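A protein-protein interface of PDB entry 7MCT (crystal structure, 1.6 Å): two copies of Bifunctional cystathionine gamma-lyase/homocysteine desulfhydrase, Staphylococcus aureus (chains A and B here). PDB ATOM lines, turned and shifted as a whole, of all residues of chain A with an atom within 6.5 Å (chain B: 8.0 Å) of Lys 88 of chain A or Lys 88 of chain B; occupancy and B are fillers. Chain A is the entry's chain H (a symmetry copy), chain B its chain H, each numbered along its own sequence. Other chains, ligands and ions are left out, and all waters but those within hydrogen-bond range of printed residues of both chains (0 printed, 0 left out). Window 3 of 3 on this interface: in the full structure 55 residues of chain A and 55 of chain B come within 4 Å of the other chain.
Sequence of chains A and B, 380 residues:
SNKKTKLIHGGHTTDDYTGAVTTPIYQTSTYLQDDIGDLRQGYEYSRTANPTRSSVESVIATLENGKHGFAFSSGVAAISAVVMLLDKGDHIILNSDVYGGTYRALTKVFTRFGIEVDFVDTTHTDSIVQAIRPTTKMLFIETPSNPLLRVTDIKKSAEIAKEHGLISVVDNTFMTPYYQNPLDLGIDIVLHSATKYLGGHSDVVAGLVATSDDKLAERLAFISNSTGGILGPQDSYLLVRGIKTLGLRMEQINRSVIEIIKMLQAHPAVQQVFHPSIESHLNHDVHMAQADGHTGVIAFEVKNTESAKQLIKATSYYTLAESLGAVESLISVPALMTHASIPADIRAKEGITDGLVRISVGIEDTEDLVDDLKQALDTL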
ATOM      1  N   LEU A  86       8.191 -33.609 -29.571  1.00  0.00           N
ATOM      2  CA  LEU A  86       7.048 -33.360 -28.697  1.00  0.00           C
ATOM      3  C   LEU A  86       7.154 -31.997 -28.016  1.00  0.00           C
ATOM      4  O   LEU A  86       8.213 -31.366 -27.988  1.00  0.00           O
ATOM      5  CB  LEU A  86       6.952 -34.462 -27.643  1.00  0.00           C
ATOM      6  CG  LEU A  86       6.914 -35.887 -28.189  1.00  0.00           C
ATOM      7  CD1 LEU A  86       6.680 -36.855 -27.063  1.00  0.00           C
ATOM      8  CD2 LEU A  86       5.849 -36.051 -29.262  1.00  0.00           C
ATOM      9  N   ASP A  87       6.031 -31.559 -27.435  1.00  0.00           N
ATOM     10  CA  ASP A  87       5.917 -30.311 -26.691  1.00  0.00           C
ATOM     11  C   ASP A  87       5.679 -30.580 -25.210  1.00  0.00           C
ATOM     12  O   ASP A  87       5.214 -31.654 -24.815  1.00  0.00           O
ATOM     13  CB  ASP A  87       4.734 -29.463 -27.178  1.00  0.00           C
ATOM     14  CG  ASP A  87       4.841 -29.048 -28.624  1.00  0.00           C
ATOM     15  OD1 ASP A  87       5.904 -29.229 -29.253  1.00  0.00           O
ATOM     16  OD2 ASP A  87       3.825 -28.539 -29.136  1.00  0.00           O
ATOM     17  N   LYS A  88       5.956 -29.563 -24.396  1.00  0.00           N
ATOM     18  CA  LYS A  88       5.503 -29.550 -23.011  1.00  0.00           C
ATOM     19  C   LYS A  88       4.049 -29.995 -22.937  1.00  0.00           C
ATOM     20  O   LYS A  88       3.219 -29.567 -23.742  1.00  0.00           O
ATOM     21  CB  LYS A  88       5.650 -28.140 -22.441  1.00  0.00           C
ATOM     22  CG  LYS A  88       4.917 -27.903 -21.146  1.00  0.00           C
ATOM     23  CD  LYS A  88       4.720 -26.413 -20.938  1.00  0.00           C
ATOM     24  N   GLY A  89       3.756 -30.902 -22.005  1.00  0.00           N
ATOM     25  CA  GLY A  89       2.415 -31.431 -21.835  1.00  0.00           C
ATOM     26  C   GLY A  89       2.135 -32.721 -22.581  1.00  0.00           C
ATOM     27  O   GLY A  89       1.146 -33.395 -22.275  1.00  0.00           O
ATOM     28  N   ASP A  90       2.973 -33.083 -23.551  1.00  0.00           N
ATOM     29  CA  ASP A  90       2.829 -34.344 -24.261  1.00  0.00           C
ATOM     30  C   ASP A  90       3.354 -35.499 -23.410  1.00  0.00           C
ATOM     31  O   ASP A  90       4.228 -35.324 -22.557  1.00  0.00           O
ATOM     32  CB  ASP A  90       3.598 -34.300 -25.590  1.00  0.00           C
ATOM     33  CG  ASP A  90       2.963 -33.370 -26.615  1.00  0.00           C
ATOM     34  OD1 ASP A  90       1.796 -32.930 -26.418  1.00  0.00           O
ATOM     35  OD2 ASP A  90       3.638 -33.079 -27.628  1.00  0.00           O
ATOM     36  N   THR A 111      11.675 -34.294 -18.461  1.00  0.00           N
ATOM     37  CA  THR A 111      10.556 -33.984 -17.566  1.00  0.00           C
ATOM     38  C   THR A 111      10.643 -32.556 -17.048  1.00  0.00           C
ATOM     39  O   THR A 111       9.613 -31.969 -16.687  1.00  0.00           O
ATOM     40  CB  THR A 111      10.488 -34.956 -16.387  1.00  0.00           C
ATOM     41  OG1 THR A 111      11.755 -35.000 -15.720  1.00  0.00           O
ATOM     42  CG2 THR A 111      10.094 -36.350 -16.858  1.00  0.00           C
ATOM     43  N   ARG A 112      11.846 -31.979 -17.001  1.00  0.00           N
ATOM     44  CA  ARG A 112      11.966 -30.576 -16.628  1.00  0.00           C
ATOM     45  C   ARG A 112      11.371 -29.663 -17.689  1.00  0.00           C
ATOM     46  O   ARG A 112      11.077 -28.500 -17.394  1.00  0.00           O
ATOM     47  CB  ARG A 112      13.428 -30.203 -16.378  1.00  0.00           C
ATOM     48  CG  ARG A 112      14.068 -30.961 -15.231  1.00  0.00           C
ATOM     49  CD  ARG A 112      15.412 -30.385 -14.854  1.00  0.00           C
ATOM     50  NE  ARG A 112      16.447 -30.686 -15.850  1.00  0.00           N
ATOM     51  CZ  ARG A 112      16.920 -29.813 -16.733  1.00  0.00           C
ATOM     52  NH1 ARG A 112      16.449 -28.575 -16.758  1.00  0.00           N
ATOM     53  NH2 ARG A 112      17.876 -30.178 -17.593  1.00  0.00           N
ATOM     54  N   PHE A 113      11.169 -30.172 -18.903  1.00  0.00           N
ATOM     55  CA  PHE A 113      10.545 -29.431 -19.986  1.00  0.00           C
ATOM     56  C   PHE A 113       9.074 -29.789 -20.159  1.00  0.00           C
ATOM     57  O   PHE A 113       8.489 -29.490 -21.205  1.00  0.00           O
ATOM     58  CB  PHE A 113      11.313 -29.661 -21.285  1.00  0.00           C
ATOM     59  CG  PHE A 113      12.759 -29.300 -21.181  1.00  0.00           C
ATOM     60  CD1 PHE A 113      13.137 -28.100 -20.609  1.00  0.00           C
ATOM     61  CD2 PHE A 113      13.738 -30.162 -21.630  1.00  0.00           C
ATOM     62  CE1 PHE A 113      14.466 -27.754 -20.492  1.00  0.00           C
ATOM     63  CE2 PHE A 113      15.071 -29.823 -21.517  1.00  0.00           C
ATOM     64  CZ  PHE A 113      15.431 -28.615 -20.941  1.00  0.00           C
ATOM     65  N   GLY A 114       8.476 -30.447 -19.171  1.00  0.00           N
ATOM     66  CA  GLY A 114       7.061 -30.746 -19.224  1.00  0.00           C
ATOM     67  C   GLY A 114       6.666 -31.955 -20.039  1.00  0.00           C
ATOM     68  O   GLY A 114       5.466 -32.179 -20.232  1.00  0.00           O
ATOM     69  N   ILE A 115       7.625 -32.733 -20.535  1.00  0.00           N
ATOM     70  CA  ILE A 115       7.304 -34.016 -21.147  1.00  0.00           C
ATOM     71  C   ILE A 115       6.964 -35.001 -20.041  1.00  0.00           C
ATOM     72  O   ILE A 115       7.686 -35.100 -19.044  1.00  0.00           O
ATOM     73  CB  ILE A 115       8.478 -34.529 -21.995  1.00  0.00           C
ATOM     74  CG1 ILE A 115       8.906 -33.461 -22.996  1.00  0.00           C
ATOM     75  CG2 ILE A 115       8.105 -35.840 -22.685  1.00  0.00           C
ATOM     76  CD1 ILE A 115       7.846 -33.144 -23.995  1.00  0.00           C
ATOM     77  N   VAL B  83      21.006 -23.647 -22.480  1.00  0.00           N
ATOM     78  CA  VAL B  83      19.588 -23.342 -22.270  1.00  0.00           C
ATOM     79  C   VAL B  83      18.924 -24.436 -21.443  1.00  0.00           C
ATOM     80  O   VAL B  83      18.041 -24.155 -20.617  1.00  0.00           O
ATOM     81  CB  VAL B  83      18.872 -23.136 -23.623  1.00  0.00           C
ATOM     82  CG1 VAL B  83      17.344 -23.061 -23.426  1.00  0.00           C
ATOM     83  CG2 VAL B  83      19.371 -21.862 -24.285  1.00  0.00           C
ATOM     84  N   MET B  84      19.358 -25.688 -21.615  1.00  0.00           N
ATOM     85  CA  MET B  84      18.795 -26.803 -20.862  1.00  0.00           C
ATOM     86  C   MET B  84      19.125 -26.772 -19.375  1.00  0.00           C
ATOM     87  O   MET B  84      18.635 -27.643 -18.641  1.00  0.00           O
ATOM     88  CB  MET B  84      19.277 -28.123 -21.459  1.00  0.00           C
ATOM     89  CG  MET B  84      18.541 -28.507 -22.717  1.00  0.00           C
ATOM     90  SD  MET B  84      19.126 -30.097 -23.303  1.00  0.00           S
ATOM     91  CE  MET B  84      17.830 -30.459 -24.438  1.00  0.00           C
ATOM     92  N   LEU B  85      19.951 -25.829 -18.915  1.00  0.00           N
ATOM     93  CA  LEU B  85      20.078 -25.583 -17.483  1.00  0.00           C
ATOM     94  C   LEU B  85      18.759 -25.137 -16.867  1.00  0.00           C
ATOM     95  O   LEU B  85      18.579 -25.263 -15.647  1.00  0.00           O
ATOM     96  CB  LEU B  85      21.140 -24.519 -17.221  1.00  0.00           C
ATOM     97  CG  LEU B  85      22.577 -24.939 -17.545  1.00  0.00           C
ATOM     98  CD1 LEU B  85      23.484 -23.725 -17.524  1.00  0.00           C
ATOM     99  CD2 LEU B  85      23.038 -25.981 -16.539  1.00  0.00           C
ATOM    100  N   LEU B  86      17.844 -24.616 -17.676  1.00  0.00           N
ATOM    101  CA  LEU B  86      16.579 -24.064 -17.201  1.00  0.00           C
ATOM    102  C   LEU B  86      15.450 -25.087 -17.309  1.00  0.00           C
ATOM    103  O   LEU B  86      15.561 -26.107 -17.993  1.00  0.00           O
ATOM    104  CB  LEU B  86      16.225 -22.813 -18.004  1.00  0.00           C
ATOM    105  CG  LEU B  86      17.305 -21.734 -18.041  1.00  0.00           C
ATOM    106  CD1 LEU B  86      16.777 -20.513 -18.740  1.00  0.00           C
ATOM    107  CD2 LEU B  86      17.795 -21.379 -16.646  1.00  0.00           C
ATOM    108  N   ASP B  87      14.333 -24.780 -16.636  1.00  0.00           N
ATOM    109  CA  ASP B  87      13.120 -25.586 -16.636  1.00  0.00           C
ATOM    110  C   ASP B  87      11.985 -24.861 -17.349  1.00  0.00           C
ATOM    111  O   ASP B  87      11.987 -23.633 -17.485  1.00  0.00           O
ATOM    112  CB  ASP B  87      12.629 -25.878 -15.211  1.00  0.00           C
ATOM    113  CG  ASP B  87      13.616 -26.657 -14.378  1.00  0.00           C
ATOM    114  OD1 ASP B  87      14.625 -27.165 -14.909  1.00  0.00           O
ATOM    115  OD2 ASP B  87      13.370 -26.746 -13.159  1.00  0.00           O
ATOM    116  N   LYS B  88      10.982 -25.636 -17.756  1.00  0.00           N
ATOM    117  CA  LYS B  88       9.703 -25.073 -18.170  1.00  0.00           C
ATOM    118  C   LYS B  88       9.265 -23.999 -17.185  1.00  0.00           C
ATOM    119  O   LYS B  88       9.363 -24.183 -15.969  1.00  0.00           O
ATOM    120  CB  LYS B  88       8.656 -26.184 -18.237  1.00  0.00           C
ATOM    121  CG  LYS B  88       7.230 -25.703 -18.322  1.00  0.00           C
ATOM    122  CD  LYS B  88       6.291 -26.815 -17.894  1.00  0.00           C
ATOM    123  N   GLY B  89       8.837 -22.853 -17.713  1.00  0.00           N
ATOM    124  CA  GLY B  89       8.409 -21.735 -16.891  1.00  0.00           C
ATOM    125  C   GLY B  89       9.485 -20.710 -16.592  1.00  0.00           C
ATOM    126  O   GLY B  89       9.159 -19.599 -16.161  1.00  0.00           O
ATOM    127  N   ASP B  90      10.755 -21.049 -16.803  1.00  0.00           N
ATOM    128  CA  ASP B  90      11.844 -20.102 -16.622  1.00  0.00           C
ATOM    129  C   ASP B  90      11.926 -19.149 -17.813  1.00  0.00           C
ATOM    130  O   ASP B  90      11.527 -19.482 -18.932  1.00  0.00           O
ATOM    131  CB  ASP B  90      13.180 -20.846 -16.472  1.00  0.00           C
ATOM    132  CG  ASP B  90      13.295 -21.603 -15.156  1.00  0.00           C
ATOM    133  OD1 ASP B  90      12.463 -21.378 -14.233  1.00  0.00           O
ATOM    134  OD2 ASP B  90      14.229 -22.430 -15.044  1.00  0.00           O
ATOM    135  N   HIS B  91      12.489 -17.972 -17.571  1.00  0.00           N
ATOM    136  CA  HIS B  91      12.563 -16.913 -18.570  1.00  0.00           C
ATOM    137  C   HIS B  91      14.016 -16.517 -18.825  1.00  0.00           C
ATOM    138  O   HIS B  91      14.838 -16.504 -17.898  1.00  0.00           O
ATOM    139  CB  HIS B  91      11.714 -15.718 -18.091  1.00  0.00           C
ATOM    140  CG  HIS B  91      11.775 -14.512 -18.975  1.00  0.00           C
ATOM    141  ND1 HIS B  91      12.502 -13.390 -18.644  1.00  0.00           N
ATOM    142  CD2 HIS B  91      11.152 -14.226 -20.144  1.00  0.00           C
ATOM    143  CE1 HIS B  91      12.351 -12.474 -19.585  1.00  0.00           C
ATOM    144  NE2 HIS B  91      11.533 -12.955 -20.506  1.00  0.00           N
ATOM    145  N   VAL B 109      12.204 -24.137 -30.910  1.00  0.00           N
ATOM    146  CA  VAL B 109      12.408 -25.365 -30.144  1.00  0.00           C
ATOM    147  C   VAL B 109      12.094 -25.150 -28.667  1.00  0.00           C
ATOM    148  O   VAL B 109      11.138 -25.719 -28.137  1.00  0.00           O
ATOM    149  CB  VAL B 109      13.835 -25.926 -30.346  1.00  0.00           C
ATOM    150  CG1 VAL B 109      14.005 -27.206 -29.535  1.00  0.00           C
ATOM    151  CG2 VAL B 109      14.084 -26.191 -31.822  1.00  0.00           C
ATOM    152  N   PHE B 110      12.860 -24.298 -27.988  1.00  0.00           N
ATOM    153  CA  PHE B 110      12.760 -24.276 -26.535  1.00  0.00           C
ATOM    154  C   PHE B 110      11.488 -23.618 -26.024  1.00  0.00           C
ATOM    155  O   PHE B 110      11.074 -23.929 -24.904  1.00  0.00           O
ATOM    156  CB  PHE B 110      13.996 -23.626 -25.939  1.00  0.00           C
ATOM    157  CG  PHE B 110      15.217 -24.492 -26.096  1.00  0.00           C
ATOM    158  CD1 PHE B 110      15.350 -25.646 -25.337  1.00  0.00           C
ATOM    159  CD2 PHE B 110      16.180 -24.196 -27.038  1.00  0.00           C
ATOM    160  CE1 PHE B 110      16.446 -26.474 -25.490  1.00  0.00           C
ATOM    161  CE2 PHE B 110      17.279 -25.028 -27.199  1.00  0.00           C
ATOM    162  CZ  PHE B 110      17.408 -26.162 -26.423  1.00  0.00           C
ATOM    163  N   THR B 111      10.834 -22.758 -26.812  1.00  0.00           N
ATOM    164  CA  THR B 111       9.533 -22.264 -26.350  1.00  0.00           C
ATOM    165  C   THR B 111       8.494 -23.375 -26.335  1.00  0.00           C
ATOM    166  O   THR B 111       7.520 -23.296 -25.574  1.00  0.00           O
ATOM    167  CB  THR B 111       9.033 -21.102 -27.211  1.00  0.00           C
ATOM    168  OG1 THR B 111       9.040 -21.482 -28.592  1.00  0.00           O
ATOM    169  CG2 THR B 111       9.895 -19.864 -27.002  1.00  0.00           C
ATOM    170  N   ARG B 112       8.674 -24.411 -27.157  1.00  0.00           N
ATOM    171  CA  ARG B 112       7.774 -25.556 -27.093  1.00  0.00           C
ATOM    172  C   ARG B 112       7.942 -26.326 -25.793  1.00  0.00           C
ATOM    173  O   ARG B 112       7.048 -27.094 -25.423  1.00  0.00           O
ATOM    174  CB  ARG B 112       7.994 -26.487 -28.285  1.00  0.00           C
ATOM    175  CG  ARG B 112       7.704 -25.846 -29.628  1.00  0.00           C
ATOM    176  CD  ARG B 112       7.682 -26.862 -30.746  1.00  0.00           C
ATOM    177  NE  ARG B 112       9.025 -27.351 -31.082  1.00  0.00           N
ATOM    178  CZ  ARG B 112       9.502 -28.541 -30.731  1.00  0.00           C
ATOM    179  NH1 ARG B 112       8.753 -29.373 -30.023  1.00  0.00           N
ATOM    180  NH2 ARG B 112      10.736 -28.903 -31.097  1.00  0.00           N
ATOM    181  N   PHE B 113       9.052 -26.120 -25.088  1.00  0.00           N
ATOM    182  CA  PHE B 113       9.306 -26.738 -23.797  1.00  0.00           C
ATOM    183  C   PHE B 113       9.015 -25.793 -22.637  1.00  0.00           C
ATOM    184  O   PHE B 113       9.462 -26.046 -21.514  1.00  0.00           O
ATOM    185  CB  PHE B 113      10.745 -27.241 -23.735  1.00  0.00           C
ATOM    186  CG  PHE B 113      11.079 -28.194 -24.836  1.00  0.00           C
ATOM    187  CD1 PHE B 113      10.222 -29.234 -25.139  1.00  0.00           C
ATOM    188  CD2 PHE B 113      12.231 -28.041 -25.580  1.00  0.00           C
ATOM    189  CE1 PHE B 113      10.506 -30.117 -26.160  1.00  0.00           C
ATOM    190  CE2 PHE B 113      12.522 -28.920 -26.603  1.00  0.00           C
ATOM    191  CZ  PHE B 113      11.651 -29.958 -26.893  1.00  0.00           C
ATOM    192  N   GLY B 114       8.303 -24.699 -22.892  1.00  0.00           N
ATOM    193  CA  GLY B 114       7.912 -23.800 -21.827  1.00  0.00           C
ATOM    194  C   GLY B 114       8.958 -22.808 -21.377  1.00  0.00           C
ATOM    195  O   GLY B 114       8.730 -22.109 -20.383  1.00  0.00           O
ATOM    196  N   ILE B 115      10.100 -22.728 -22.057  1.00  0.00           N
ATOM    197  CA  ILE B 115      11.050 -21.655 -21.798  1.00  0.00           C
ATOM    198  C   ILE B 115      10.503 -20.374 -22.407  1.00  0.00           C
ATOM    199  O   ILE B 115      10.057 -20.367 -23.559  1.00  0.00           O
ATOM    200  CB  ILE B 115      12.431 -21.991 -22.381  1.00  0.00           C
ATOM    201  CG1 ILE B 115      12.893 -23.355 -21.878  1.00  0.00           C
ATOM    202  CG2 ILE B 115      13.436 -20.890 -22.044  1.00  0.00           C
ATOM    203  CD1 ILE B 115      13.103 -23.389 -20.403  1.00  0.00           C
ATOM    204  N   GLU B 116      10.524 -19.293 -21.637  1.00  0.00           N
ATOM    205  CA  GLU B 116      10.062 -17.996 -22.115  1.00  0.00           C
ATOM    206  C   GLU B 116      11.261 -17.115 -22.422  1.00  0.00           C
ATOM    207  O   GLU B 116      12.265 -17.151 -21.705  1.00  0.00           O
ATOM    208  CB  GLU B 116       9.164 -17.318 -21.079  1.00  0.00           C
ATOM    209  CG  GLU B 116       8.012 -18.179 -20.604  1.00  0.00           C
ATOM    210  CD  GLU B 116       6.878 -18.232 -21.612  1.00  0.00           C
ATOM    211  OE1 GLU B 116       6.993 -17.575 -22.669  1.00  0.00           O
ATOM    212  OE2 GLU B 116       5.862 -18.905 -21.335  1.00  0.00           O
ATOM    213  N   THR B 135      10.186 -14.711 -13.020  1.00  0.00           N
ATOM    214  CA  THR B 135      10.599 -16.009 -13.534  1.00  0.00           C
ATOM    215  C   THR B 135      11.920 -15.972 -14.296  1.00  0.00           C
ATOM    216  O   THR B 135      12.384 -17.033 -14.726  1.00  0.00           O
ATOM    217  CB  THR B 135       9.522 -16.573 -14.459  1.00  0.00           C
ATOM    218  OG1 THR B 135       9.226 -15.602 -15.473  1.00  0.00           O
ATOM    219  CG2 THR B 135       8.243 -16.895 -13.672  1.00  0.00           C
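Of the printed residues of chain B, Lys 88 of chain A touches Lys 88 and Arg 112. Of chain A, only Lys 88 and Arg 112 come within 4 Å of Lys 88 of chain B. Of the printed residues of chain A, Met 84 of chain B touches Arg 112 (2.8 Å) and Phe 113 (3.6 Å). Printed residues of chain A within 4 Å of Arg 112 of chain B: Leu 86, Asp 87 and Lys 88. Of the printed residues of chain A, Asp 87 of chain B touches Arg 112. The nearest residue of chain A that does not touch Lys 88 of chain B is Phe 113 of chain A (4.1 Å).
The guanidinium group of Arg 112 of chain A lies within hydrogen-bond range of the backbone carbonyl oxygen of Leu 86 of chain B. The backbone NH of Lys 88 of chain B is in hydrogen-bond range of the backbone carbonyl oxygen of Arg 112 of chain A (2.9 Å). The backbone carbonyl oxygen (O) of Arg 112 of chain B is in hydrogen-bond range of the backbone NH (N) of Lys 88 of chain A (2.9 Å). O of Met 84 of chain B sits at hydrogen-bond distance from NH2 of Arg 112 of chain A. The side-chain carboxylate (OD1) of Asp 87 of chain B lies within salt-bridge range of the guanidinium group (NH1) of Arg 112 of chain A (3.0 Å). NH1 of Arg 112 of chain B lies within hydrogen-bond range of O of Leu 86 of chain A (2.9 Å). The side-chain carboxylate (OD1) of Asp 87 of chain A lies within salt-bridge range of the guanidinium group (NH1) of Arg 112 of chain B.
N of Asp 87 of chain A sits at hydrogen-bond distance from OD2 of Asp 90 of chain A, 2.8 Å away. The backbone NH of Asp 87 of chain B sits at hydrogen-bond distance from the side-chain carboxylate of Asp 90 of chain B (2.8 Å).
Leu 86 of chain A touches Arg 112 of chain B, and with the chains exchanged Arg 112 of chain A touches Leu 86 of chain B. Asp 87 of chain A touches Arg 112 of chain B, and with the chains exchanged Arg 112 of chain A touches Asp 87 of chain B. Lys 88 of chain B touches its own counterpart, Lys 88 of chain A. Lys 88 of chain A touches Arg 112 of chain B, and with the chains exchanged Arg 112 of chain A touches Lys 88 of chain B. 10 positions are printed for both chains.
Among the printed residues, pairs that only touch across the chains: Leu 86 of chain A with Phe 113 of chain B (3.2 Å), Lys 88 of chain A with Lys 88 of chain B (3.4 Å), Phe 113 of chain A with Met 84 of chain B (3.6 Å), Phe 113 of chain A with Leu 86 of chain B (3.2 Å) and Phe 113 of chain A with Phe 113 of chain B (3.5 Å).
Of the 18 printed residues of chain B, 6 touch a printed residue of chain A. Printed residues of chain B that touch a printed residue of chain A: Met 84, Leu 86, Asp 87, Lys 88, Arg 112 and Phe 113. Hydrophobic or aromatic side chains of chain A that line the printed part of chain B: Phe 113. Among the printed residues, 12 pairs touch across the chains.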
